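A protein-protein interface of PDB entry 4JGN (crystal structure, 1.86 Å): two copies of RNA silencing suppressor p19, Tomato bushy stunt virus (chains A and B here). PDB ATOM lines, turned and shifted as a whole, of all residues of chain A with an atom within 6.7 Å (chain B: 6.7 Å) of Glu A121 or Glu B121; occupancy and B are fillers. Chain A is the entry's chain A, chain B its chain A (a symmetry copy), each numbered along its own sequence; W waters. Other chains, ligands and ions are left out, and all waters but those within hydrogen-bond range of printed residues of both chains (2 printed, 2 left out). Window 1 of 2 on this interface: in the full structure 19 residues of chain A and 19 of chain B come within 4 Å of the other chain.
OE2 of Glu A121 lies close to OE2 of Glu B121, at 3.0 Å.
O of Met B114 is in hydrogen-bond range of OG of Ser B118 (2.8 Å).
O of Glu A113 is in hydrogen-bond range of NH1 of Arg A117 (2.8 Å).
O of Met A114 sits at hydrogen-bond distance from OG of Ser A118 (2.8 Å).
NH1 of Arg B117 sits at hydrogen-bond distance from O of Glu B113 (2.8 Å).
Among the printed residues, merely in contact across the chains: Ile A99 with Ile B99, Glu A113 with Leu B125, Met A114 with Glu B121, Met A114 with Leu B122, Met A114 with Leu B125, Arg A117 with Glu B121, Glu A121 with Met B114, Glu A121 with Arg B117, Leu A122 with Met B114, Leu A125 with Glu B113 and Leu A125 with Met B114.
Glu A121 touches three residues of chain B.
Gln A124 touches none of the printed residues of chain B.
Of the printed residues of chain A, Met B114 touches Glu A121 (3.9 Å), Leu A122 (3.8 Å) and Leu A125 (2.9 Å).
Of chain A, only Met A114 (3.9 Å), Arg A117 (3.2 Å) and Glu A121 (3.0 Å) come within 4 Å of Glu B121.
Of the printed residues of chain A, Leu B122 touches Met A114.
The nearest residue of chain B that does not touch Glu A121 is Ser B118 (4.8 Å).
The nearest printed residue of chain A that does not touch Glu B113 is Ala A126 (4.7 Å).
Hydrophobic or aromatic side chains of chain B that line the printed part of chain A: Ile B99, Met B114, Leu B122 and Leu B125.
Of the 15 printed residues of chain A, 7 touch a printed residue of chain B.
Printed residues of chain A that touch a printed residue of chain B: Ile A99, Glu A113, Met A114, Arg A117, Glu A121, Leu A122 and Leu A125.
Hydrophobic or aromatic side chains of chain A within 4 Å of the printed part of chain B: Ile A99, Met A114, Leu A122 and Leu A125.
Among the printed residues, no Asp or Glu carboxylate lies within 4 Å of a Lys or Arg side-chain nitrogen of the other chain.
Glu A113 touches Leu B125, and with the chains exchanged Leu A125 touches Glu B113.
Met A114 touches Glu B121, and with the chains exchanged Glu A121 touches Met B114.
Met A114 touches Leu B122, and with the chains exchanged Leu A122 touches Met B114.
Met A114 touches Leu B125, and with the chains exchanged Leu A125 touches Met B114.
Positions printed for both chains: 65, 99, 113, 114, 116, 117, 118, 119, 120, 121, 122, 123, 124, 125 and 126.
Water W1 bridges the side-chain carboxylate of Glu B121 and the backbone carbonyl oxygen of Arg A117.
Water W2 lies within hydrogen-bond range of OE2 of Glu A121 (2.5 Å) and O of Arg B117 (3.2 Å).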
ATOM      1  N   LEU A  65     -26.975 -13.203  -7.454  1.00  0.00           N
ATOM      2  CA  LEU A  65     -27.209 -13.614  -6.110  1.00  0.00           C
ATOM      3  C   LEU A  65     -27.525 -15.118  -6.108  1.00  0.00           C
ATOM      4  O   LEU A  65     -27.471 -15.753  -5.036  1.00  0.00           O
ATOM      5  CB  LEU A  65     -28.425 -12.897  -5.518  1.00  0.00           C
ATOM      6  CG  LEU A  65     -28.275 -11.636  -4.680  1.00  0.00           C
ATOM      7  CD1 LEU A  65     -26.902 -11.253  -4.117  1.00  0.00           C
ATOM      8  CD2 LEU A  65     -29.252 -10.513  -4.852  1.00  0.00           C
ATOM      9  N   ILE A  99     -15.091  -7.009   0.431  1.00  0.00           N
ATOM     10  CA  ILE A  99     -15.612  -7.406   1.758  1.00  0.00           C
ATOM     11  C   ILE A  99     -15.189  -8.888   1.944  1.00  0.00           C
ATOM     12  O   ILE A  99     -15.300  -9.694   1.000  1.00  0.00           O
ATOM     13  CB  ILE A  99     -17.176  -7.282   1.815  1.00  0.00           C
ATOM     14  CG1 ILE A  99     -17.542  -5.790   1.540  1.00  0.00           C
ATOM     15  CG2 ILE A  99     -17.736  -7.764   3.236  1.00  0.00           C
ATOM     16  CD1 ILE A  99     -19.156  -5.469   1.588  1.00  0.00           C
ATOM     17  N   GLU A 113     -24.889 -16.460   6.012  1.00  0.00           N
ATOM     18  CA  GLU A 113     -25.925 -15.457   6.204  1.00  0.00           C
ATOM     19  C   GLU A 113     -25.364 -14.025   6.059  1.00  0.00           C
ATOM     20  O   GLU A 113     -25.998 -13.102   5.428  1.00  0.00           O
ATOM     21  CB  GLU A 113     -26.520 -15.644   7.642  1.00  0.00           C
ATOM     22  CG  GLU A 113     -27.388 -16.835   7.737  1.00  0.00           C
ATOM     23  CD  GLU A 113     -27.773 -17.293   9.193  1.00  0.00           C
ATOM     24  OE1 GLU A 113     -28.453 -18.340   9.241  1.00  0.00           O
ATOM     25  OE2 GLU A 113     -27.411 -16.690  10.264  1.00  0.00           O
ATOM     26  N   MET A 114     -24.215 -13.835   6.683  1.00  0.00           N
ATOM     27  CA  MET A 114     -23.505 -12.558   6.564  1.00  0.00           C
ATOM     28  C   MET A 114     -22.889 -12.348   5.164  1.00  0.00           C
ATOM     29  O   MET A 114     -22.910 -11.229   4.646  1.00  0.00           O
ATOM     30  CB  MET A 114     -22.389 -12.457   7.590  1.00  0.00           C
ATOM     31  CG  MET A 114     -22.810 -12.317   9.051  1.00  0.00           C
ATOM     32  SD  MET A 114     -23.915 -10.822   9.204  1.00  0.00           S
ATOM     33  CE  MET A 114     -25.392 -11.657   9.531  1.00  0.00           C
ATOM     34  N   ILE A 116     -24.125 -13.505   2.233  1.00  0.00           N
ATOM     35  CA  ILE A 116     -25.174 -13.141   1.257  1.00  0.00           C
ATOM     36  C   ILE A 116     -25.684 -11.731   1.434  1.00  0.00           C
ATOM     37  O   ILE A 116     -26.023 -11.065   0.480  1.00  0.00           O
ATOM     38  CB  ILE A 116     -26.363 -14.147   1.227  1.00  0.00           C
ATOM     39  CG1 ILE A 116     -27.171 -13.941  -0.036  1.00  0.00           C
ATOM     40  CG2 ILE A 116     -27.240 -14.124   2.477  1.00  0.00           C
ATOM     41  CD1 ILE A 116     -26.485 -14.429  -1.164  1.00  0.00           C
ATOM     42  N   ARG A 117     -25.751 -11.294   2.683  1.00  0.00           N
ATOM     43  CA  ARG A 117     -26.160  -9.892   2.941  1.00  0.00           C
ATOM     44  C   ARG A 117     -25.088  -8.907   2.509  1.00  0.00           C
ATOM     45  O   ARG A 117     -25.421  -7.841   1.947  1.00  0.00           O
ATOM     46  CB  ARG A 117     -26.431  -9.704   4.436  1.00  0.00           C
ATOM     47  CG  ARG A 117     -27.707 -10.387   4.909  1.00  0.00           C
ATOM     48  CD  ARG A 117     -27.777 -10.414   6.499  1.00  0.00           C
ATOM     49  NE  ARG A 117     -28.938 -11.093   7.117  1.00  0.00           N
ATOM     50  CZ  ARG A 117     -29.319 -12.368   6.898  1.00  0.00           C
ATOM     51  NH1 ARG A 117     -28.724 -13.178   5.994  1.00  0.00           N
ATOM     52  NH2 ARG A 117     -30.363 -12.839   7.565  1.00  0.00           N
ATOM     53  N   SER A 118     -23.812  -9.257   2.712  1.00  0.00           N
ATOM     54  CA  SER A 118     -22.719  -8.374   2.258  1.00  0.00           C
ATOM     55  C   SER A 118     -22.692  -8.213   0.721  1.00  0.00           C
ATOM     56  O   SER A 118     -22.463  -7.112   0.196  1.00  0.00           O
ATOM     57  CB  SER A 118     -21.329  -8.889   2.675  1.00  0.00           C
ATOM     58  OG  SER A 118     -21.199  -9.053   4.105  1.00  0.00           O
ATOM     59  N   LYS A 119     -22.840  -9.342   0.057  1.00  0.00           N
ATOM     60  CA  LYS A 119     -22.932  -9.404  -1.377  1.00  0.00           C
ATOM     61  C   LYS A 119     -24.057  -8.539  -1.878  1.00  0.00           C
ATOM     62  O   LYS A 119     -23.845  -7.683  -2.737  1.00  0.00           O
ATOM     63  CB  LYS A 119     -23.150 -10.909  -1.792  1.00  0.00           C
ATOM     64  CG  LYS A 119     -23.207 -11.056  -3.331  1.00  0.00           C
ATOM     65  CD  LYS A 119     -23.288 -12.566  -3.645  1.00  0.00           C
ATOM     66  CE  LYS A 119     -23.215 -12.674  -5.156  1.00  0.00           C
ATOM     67  NZ  LYS A 119     -23.030 -14.216  -5.454  1.00  0.00           N
ATOM     68  N   GLN A 120     -25.227  -8.652  -1.295  1.00  0.00           N
ATOM     69  CA  GLN A 120     -26.323  -7.847  -1.816  1.00  0.00           C
ATOM     70  C   GLN A 120     -26.143  -6.328  -1.603  1.00  0.00           C
ATOM     71  O   GLN A 120     -26.383  -5.486  -2.549  1.00  0.00           O
ATOM     72  CB  GLN A 120     -27.646  -8.218  -1.170  1.00  0.00           C
ATOM     73  CG  GLN A 120     -27.938  -9.672  -1.142  1.00  0.00           C
ATOM     74  CD  GLN A 120     -29.237 -10.014  -0.394  1.00  0.00           C
ATOM     75  OE1 GLN A 120     -30.304  -9.411  -0.671  1.00  0.00           O
ATOM     76  NE2 GLN A 120     -29.165 -10.987   0.523  1.00  0.00           N
ATOM     77  N   GLU A 121     -25.641  -5.967  -0.420  1.00  0.00           N
ATOM     78  CA  GLU A 121     -25.381  -4.525  -0.114  1.00  0.00           C
ATOM     79  C   GLU A 121     -24.312  -3.993  -1.002  1.00  0.00           C
ATOM     80  O   GLU A 121     -24.475  -2.885  -1.557  1.00  0.00           O
ATOM     81  CB  GLU A 121     -25.000  -4.375   1.369  1.00  0.00           C
ATOM     82  CG  GLU A 121     -26.204  -4.906   2.142  1.00  0.00           C
ATOM     83  CD  GLU A 121     -26.619  -4.092   3.345  1.00  0.00           C
ATOM     84  OE1 GLU A 121     -27.706  -3.430   3.313  1.00  0.00           O
ATOM     85  OE2 GLU A 121     -25.855  -4.145   4.333  1.00  0.00           O
ATOM     86  N   LEU A 122     -23.216  -4.748  -1.179  1.00  0.00           N
ATOM     87  CA  LEU A 122     -22.179  -4.215  -2.019  1.00  0.00           C
ATOM     88  C   LEU A 122     -22.607  -4.039  -3.483  1.00  0.00           C
ATOM     89  O   LEU A 122     -22.310  -3.025  -4.137  1.00  0.00           O
ATOM     90  CB  LEU A 122     -20.957  -5.152  -1.963  1.00  0.00           C
ATOM     91  CG  LEU A 122     -19.759  -4.650  -2.785  1.00  0.00           C
ATOM     92  CD1 LEU A 122     -19.274  -3.240  -2.303  1.00  0.00           C
ATOM     93  CD2 LEU A 122     -18.627  -5.671  -2.699  1.00  0.00           C
ATOM     94  N   LEU A 123     -23.323  -5.033  -3.992  1.00  0.00           N
ATOM     95  CA  LEU A 123     -23.699  -4.950  -5.413  1.00  0.00           C
ATOM     96  C   LEU A 123     -24.753  -3.844  -5.616  1.00  0.00           C
ATOM     97  O   LEU A 123     -24.916  -3.411  -6.730  1.00  0.00           O
ATOM     98  CB  LEU A 123     -24.281  -6.257  -5.851  1.00  0.00           C
ATOM     99  CG  LEU A 123     -23.159  -7.288  -5.905  1.00  0.00           C
ATOM    100  CD1 LEU A 123     -23.724  -8.772  -6.380  1.00  0.00           C
ATOM    101  CD2 LEU A 123     -21.943  -6.931  -6.720  1.00  0.00           C
ATOM    102  N   GLN A 124     -25.427  -3.415  -4.540  1.00  0.00           N
ATOM    103  CA  GLN A 124     -26.454  -2.396  -4.687  1.00  0.00           C
ATOM    104  C   GLN A 124     -25.972  -1.045  -4.291  1.00  0.00           C
ATOM    105  O   GLN A 124     -26.748  -0.068  -4.397  1.00  0.00           O
ATOM    106  CB  GLN A 124     -27.688  -2.736  -3.883  1.00  0.00           C
ATOM    107  CG  GLN A 124     -28.426  -3.900  -4.408  1.00  0.00           C
ATOM    108  CD  GLN A 124     -29.687  -4.170  -3.616  1.00  0.00           C
ATOM    109  OE1 GLN A 124     -30.785  -4.115  -4.165  1.00  0.00           O
ATOM    110  NE2 GLN A 124     -29.549  -4.412  -2.333  1.00  0.00           N
ATOM    111  N   LEU A 125     -24.706  -0.953  -3.890  1.00  0.00           N
ATOM    112  CA  LEU A 125     -24.154   0.308  -3.396  1.00  0.00           C
ATOM    113  C   LEU A 125     -24.342   1.417  -4.398  1.00  0.00           C
ATOM    114  O   LEU A 125     -24.044   1.209  -5.556  1.00  0.00           O
ATOM    115  CB  LEU A 125     -22.657   0.165  -3.144  1.00  0.00           C
ATOM    116  CG  LEU A 125     -22.049   1.308  -2.283  1.00  0.00           C
ATOM    117  CD1 LEU A 125     -22.949   1.760  -1.061  1.00  0.00           C
ATOM    118  CD2 LEU A 125     -20.643   0.889  -1.836  1.00  0.00           C
ATOM    119  N   ALA A 126     -24.800   2.604  -3.948  1.00  0.00           N
ATOM    120  CA  ALA A 126     -24.938   3.761  -4.848  1.00  0.00           C
ATOM    121  C   ALA A 126     -23.546   4.091  -5.412  1.00  0.00           C
ATOM    122  O   ALA A 126     -22.553   3.997  -4.698  1.00  0.00           O
ATOM    123  CB  ALA A 126     -25.552   4.950  -4.118  1.00  0.00           C
ATOM    124  N   LEU B  65     -23.201   1.701  17.536  1.00  0.00           N
ATOM    125  CA  LEU B  65     -23.173   2.168  16.190  1.00  0.00           C
ATOM    126  C   LEU B  65     -22.690   3.627  16.190  1.00  0.00           C
ATOM    127  O   LEU B  65     -22.304   4.144  15.122  1.00  0.00           O
ATOM    128  CB  LEU B  65     -24.573   2.156  15.573  1.00  0.00           C
ATOM    129  CG  LEU B  65     -25.062   0.987  14.731  1.00  0.00           C
ATOM    130  CD1 LEU B  65     -24.057  -0.037  14.192  1.00  0.00           C
ATOM    131  CD2 LEU B  65     -26.474   0.508  14.880  1.00  0.00           C
ATOM    132  N   ILE B  99     -15.899  -9.665   9.838  1.00  0.00           N
ATOM    133  CA  ILE B  99     -16.126  -9.067   8.504  1.00  0.00           C
ATOM    134  C   ILE B  99     -15.012  -7.998   8.334  1.00  0.00           C
ATOM    135  O   ILE B  99     -14.720  -7.243   9.279  1.00  0.00           O
ATOM    136  CB  ILE B  99     -17.539  -8.388   8.419  1.00  0.00           C
ATOM    137  CG1 ILE B  99     -18.610  -9.493   8.680  1.00  0.00           C
ATOM    138  CG2 ILE B  99     -17.754  -7.697   6.989  1.00  0.00           C
ATOM    139  CD1 ILE B  99     -20.165  -8.959   8.600  1.00  0.00           C
ATOM    140  N   GLU B 113     -19.515   3.402   4.127  1.00  0.00           N
ATOM    141  CA  GLU B 113     -20.912   3.055   3.911  1.00  0.00           C
ATOM    142  C   GLU B 113     -21.149   1.536   4.059  1.00  0.00           C
ATOM    143  O   GLU B 113     -22.173   1.060   4.674  1.00  0.00           O
ATOM    144  CB  GLU B 113     -21.305   3.508   2.464  1.00  0.00           C
ATOM    145  CG  GLU B 113     -21.456   4.974   2.358  1.00  0.00           C
ATOM    146  CD  GLU B 113     -21.531   5.557   0.897  1.00  0.00           C
ATOM    147  OE1 GLU B 113     -21.592   6.803   0.842  1.00  0.00           O
ATOM    148  OE2 GLU B 113     -21.502   4.848  -0.170  1.00  0.00           O
ATOM    149  N   MET B 114     -20.240   0.791   3.455  1.00  0.00           N
ATOM    150  CA  MET B 114     -20.271  -0.669   3.581  1.00  0.00           C
ATOM    151  C   MET B 114     -19.869  -1.154   4.990  1.00  0.00           C
ATOM    152  O   MET B 114     -20.459  -2.108   5.502  1.00  0.00           O
ATOM    153  CB  MET B 114     -19.337  -1.322   2.575  1.00  0.00           C
ATOM    154  CG  MET B 114     -19.746  -1.239   1.105  1.00  0.00           C
ATOM    155  SD  MET B 114     -21.449  -1.977   0.925  1.00  0.00           S
ATOM    156  CE  MET B 114     -22.300  -0.514   0.576  1.00  0.00           C
ATOM    157  N   ILE B 116     -20.410   0.482   7.905  1.00  0.00           N
ATOM    158  CA  ILE B 116     -21.517   0.700   8.859  1.00  0.00           C
ATOM    159  C   ILE B 116     -22.663  -0.264   8.666  1.00  0.00           C
ATOM    160  O   ILE B 116     -23.308  -0.664   9.611  1.00  0.00           O
ATOM    161  CB  ILE B 116     -22.040   2.168   8.873  1.00  0.00           C
ATOM    162  CG1 ILE B 116     -22.864   2.401  10.119  1.00  0.00           C
ATOM    163  CG2 ILE B 116     -22.787   2.582   7.607  1.00  0.00           C
ATOM    164  CD1 ILE B 116     -22.046   2.485  11.262  1.00  0.00           C
ATOM    165  N   ARG B 117     -22.918  -0.614   7.414  1.00  0.00           N
ATOM    166  CA  ARG B 117     -23.971  -1.622   7.141  1.00  0.00           C
ATOM    167  C   ARG B 117     -23.548  -3.010   7.588  1.00  0.00           C
ATOM    168  O   ARG B 117     -24.382  -3.762   8.139  1.00  0.00           O
ATOM    169  CB  ARG B 117     -24.272  -1.656   5.641  1.00  0.00           C
ATOM    170  CG  ARG B 117     -25.024  -0.426   5.148  1.00  0.00           C
ATOM    171  CD  ARG B 117     -25.041  -0.375   3.557  1.00  0.00           C
ATOM    172  NE  ARG B 117     -25.692   0.792   2.921  1.00  0.00           N
ATOM    173  CZ  ARG B 117     -25.386   2.088   3.140  1.00  0.00           C
ATOM    174  NH1 ARG B 117     -24.481   2.493   4.058  1.00  0.00           N
ATOM    175  NH2 ARG B 117     -26.039   3.016   2.456  1.00  0.00           N
ATOM    176  N   SER B 118     -22.264  -3.349   7.410  1.00  0.00           N
ATOM    177  CA  SER B 118     -21.772  -4.660   7.879  1.00  0.00           C
ATOM    178  C   SER B 118     -21.858  -4.805   9.416  1.00  0.00           C
ATOM    179  O   SER B 118     -22.223  -5.869   9.940  1.00  0.00           O
ATOM    180  CB  SER B 118     -20.306  -4.916   7.491  1.00  0.00           C
ATOM    181  OG  SER B 118     -20.084  -4.846   6.064  1.00  0.00           O
ATOM    182  N   LYS B 119     -21.431  -3.751  10.083  1.00  0.00           N
ATOM    183  CA  LYS B 119     -21.505  -3.644  11.515  1.00  0.00           C
ATOM    184  C   LYS B 119     -22.922  -3.824  11.991  1.00  0.00           C
ATOM    185  O   LYS B 119     -23.184  -4.667  12.850  1.00  0.00           O
ATOM    186  CB  LYS B 119     -20.944  -2.232  11.933  1.00  0.00           C
ATOM    187  CG  LYS B 119     -20.949  -2.069  13.472  1.00  0.00           C
ATOM    188  CD  LYS B 119     -20.265  -0.722  13.792  1.00  0.00           C
ATOM    189  CE  LYS B 119     -20.175  -0.656  15.304  1.00  0.00           C
ATOM    190  NZ  LYS B 119     -19.246   0.585  15.613  1.00  0.00           N
ATOM    191  N   GLN B 120     -23.866  -3.142  11.388  1.00  0.00           N
ATOM    192  CA  GLN B 120     -25.227  -3.284  11.885  1.00  0.00           C
ATOM    193  C   GLN B 120     -25.831  -4.688  11.668  1.00  0.00           C
ATOM    194  O   GLN B 120     -26.479  -5.291  12.605  1.00  0.00           O
ATOM    195  CB  GLN B 120     -26.172  -2.301  11.216  1.00  0.00           C
ATOM    196  CG  GLN B 120     -25.694  -0.899  11.190  1.00  0.00           C
ATOM    197  CD  GLN B 120     -26.631   0.047  10.420  1.00  0.00           C
ATOM    198  OE1 GLN B 120     -27.860   0.063  10.675  1.00  0.00           O
ATOM    199  NE2 GLN B 120     -26.063   0.847   9.509  1.00  0.00           N
ATOM    200  N   GLU B 121     -25.556  -5.259  10.492  1.00  0.00           N
ATOM    201  CA  GLU B 121     -26.052  -6.637  10.184  1.00  0.00           C
ATOM    202  C   GLU B 121     -25.411  -7.631  11.089  1.00  0.00           C
ATOM    203  O   GLU B 121     -26.119  -8.504  11.635  1.00  0.00           O
ATOM    204  CB  GLU B 121     -25.770  -6.966   8.707  1.00  0.00           C
ATOM    205  CG  GLU B 121     -26.530  -5.906   7.915  1.00  0.00           C
ATOM    206  CD  GLU B 121     -27.277  -6.407   6.701  1.00  0.00           C
ATOM    207  OE1 GLU B 121     -28.550  -6.433   6.709  1.00  0.00           O
ATOM    208  OE2 GLU B 121     -26.571  -6.750   5.727  1.00  0.00           O
ATOM    209  N   LEU B 122     -24.088  -7.528  11.289  1.00  0.00           N
ATOM    210  CA  LEU B 122     -23.474  -8.506  12.145  1.00  0.00           C
ATOM    211  C   LEU B 122     -23.960  -8.435  13.600  1.00  0.00           C
ATOM    212  O   LEU B 122     -24.224  -9.459  14.255  1.00  0.00           O
ATOM    213  CB  LEU B 122     -21.946  -8.311  12.116  1.00  0.00           C
ATOM    214  CG  LEU B 122     -21.178  -9.342  12.957  1.00  0.00           C
ATOM    215  CD1 LEU B 122     -21.459 -10.807  12.477  1.00  0.00           C
ATOM    216  CD2 LEU B 122     -19.685  -9.029  12.897  1.00  0.00           C
ATOM    217  N   LEU B 123     -24.088  -7.214  14.101  1.00  0.00           N
ATOM    218  CA  LEU B 123     -24.480  -7.090  15.515  1.00  0.00           C
ATOM    219  C   LEU B 123     -25.951  -7.515  15.693  1.00  0.00           C
ATOM    220  O   LEU B 123     -26.331  -7.802  16.802  1.00  0.00           O
ATOM    221  CB  LEU B 123     -24.335  -5.666  15.948  1.00  0.00           C
ATOM    222  CG  LEU B 123     -22.848  -5.337  16.028  1.00  0.00           C
ATOM    223  CD1 LEU B 123     -22.599  -3.768  16.500  1.00  0.00           C
ATOM    224  CD2 LEU B 123     -21.990  -6.253  16.863  1.00  0.00           C
ATOM    225  N   GLN B 124     -26.729  -7.553  14.603  1.00  0.00           N
ATOM    226  CA  GLN B 124     -28.132  -7.916  14.725  1.00  0.00           C
ATOM    227  C   GLN B 124     -28.388  -9.329  14.332  1.00  0.00           C
ATOM    228  O   GLN B 124     -29.551  -9.783  14.419  1.00  0.00           O
ATOM    229  CB  GLN B 124     -29.014  -7.006  13.901  1.00  0.00           C
ATOM    230  CG  GLN B 124     -29.074  -5.626  14.419  1.00  0.00           C
ATOM    231  CD  GLN B 124     -30.015  -4.763  13.605  1.00  0.00           C
ATOM    232  OE1 GLN B 124     -31.003  -4.256  14.134  1.00  0.00           O
ATOM    233  NE2 GLN B 124     -29.752  -4.630  12.326  1.00  0.00           N
ATOM    234  N   LEU B 125     -27.332 -10.047  13.954  1.00  0.00           N
ATOM    235  CA  LEU B 125     -27.481 -11.417  13.464  1.00  0.00           C
ATOM    236  C   LEU B 125     -28.218 -12.276  14.457  1.00  0.00           C
ATOM    237  O   LEU B 125     -27.877 -12.240  15.621  1.00  0.00           O
ATOM    238  CB  LEU B 125     -26.109 -12.047  13.239  1.00  0.00           C
ATOM    239  CG  LEU B 125     -26.143 -13.345  12.384  1.00  0.00           C
ATOM    240  CD1 LEU B 125     -27.125 -13.289  11.144  1.00  0.00           C
ATOM    241  CD2 LEU B 125     -24.709 -13.691  11.965  1.00  0.00           C
ATOM    242  N   ALA B 126     -29.202 -13.073  13.993  1.00  0.00           N
ATOM    243  CA  ALA B 126     -29.919 -14.000  14.884  1.00  0.00           C
ATOM    244  C   ALA B 126     -28.893 -14.983  15.472  1.00  0.00           C
ATOM    245  O   ALA B 126     -27.974 -15.404  14.777  1.00  0.00           O
ATOM    246  CB  ALA B 126     -31.034 -14.723  14.138  1.00  0.00           C
HETATM  247  O   HOH W   1     -27.967  -7.217   3.701  1.00  0.00           O
HETATM  248  O   HOH W   2     -26.863  -3.029   6.336  1.00  0.00           O
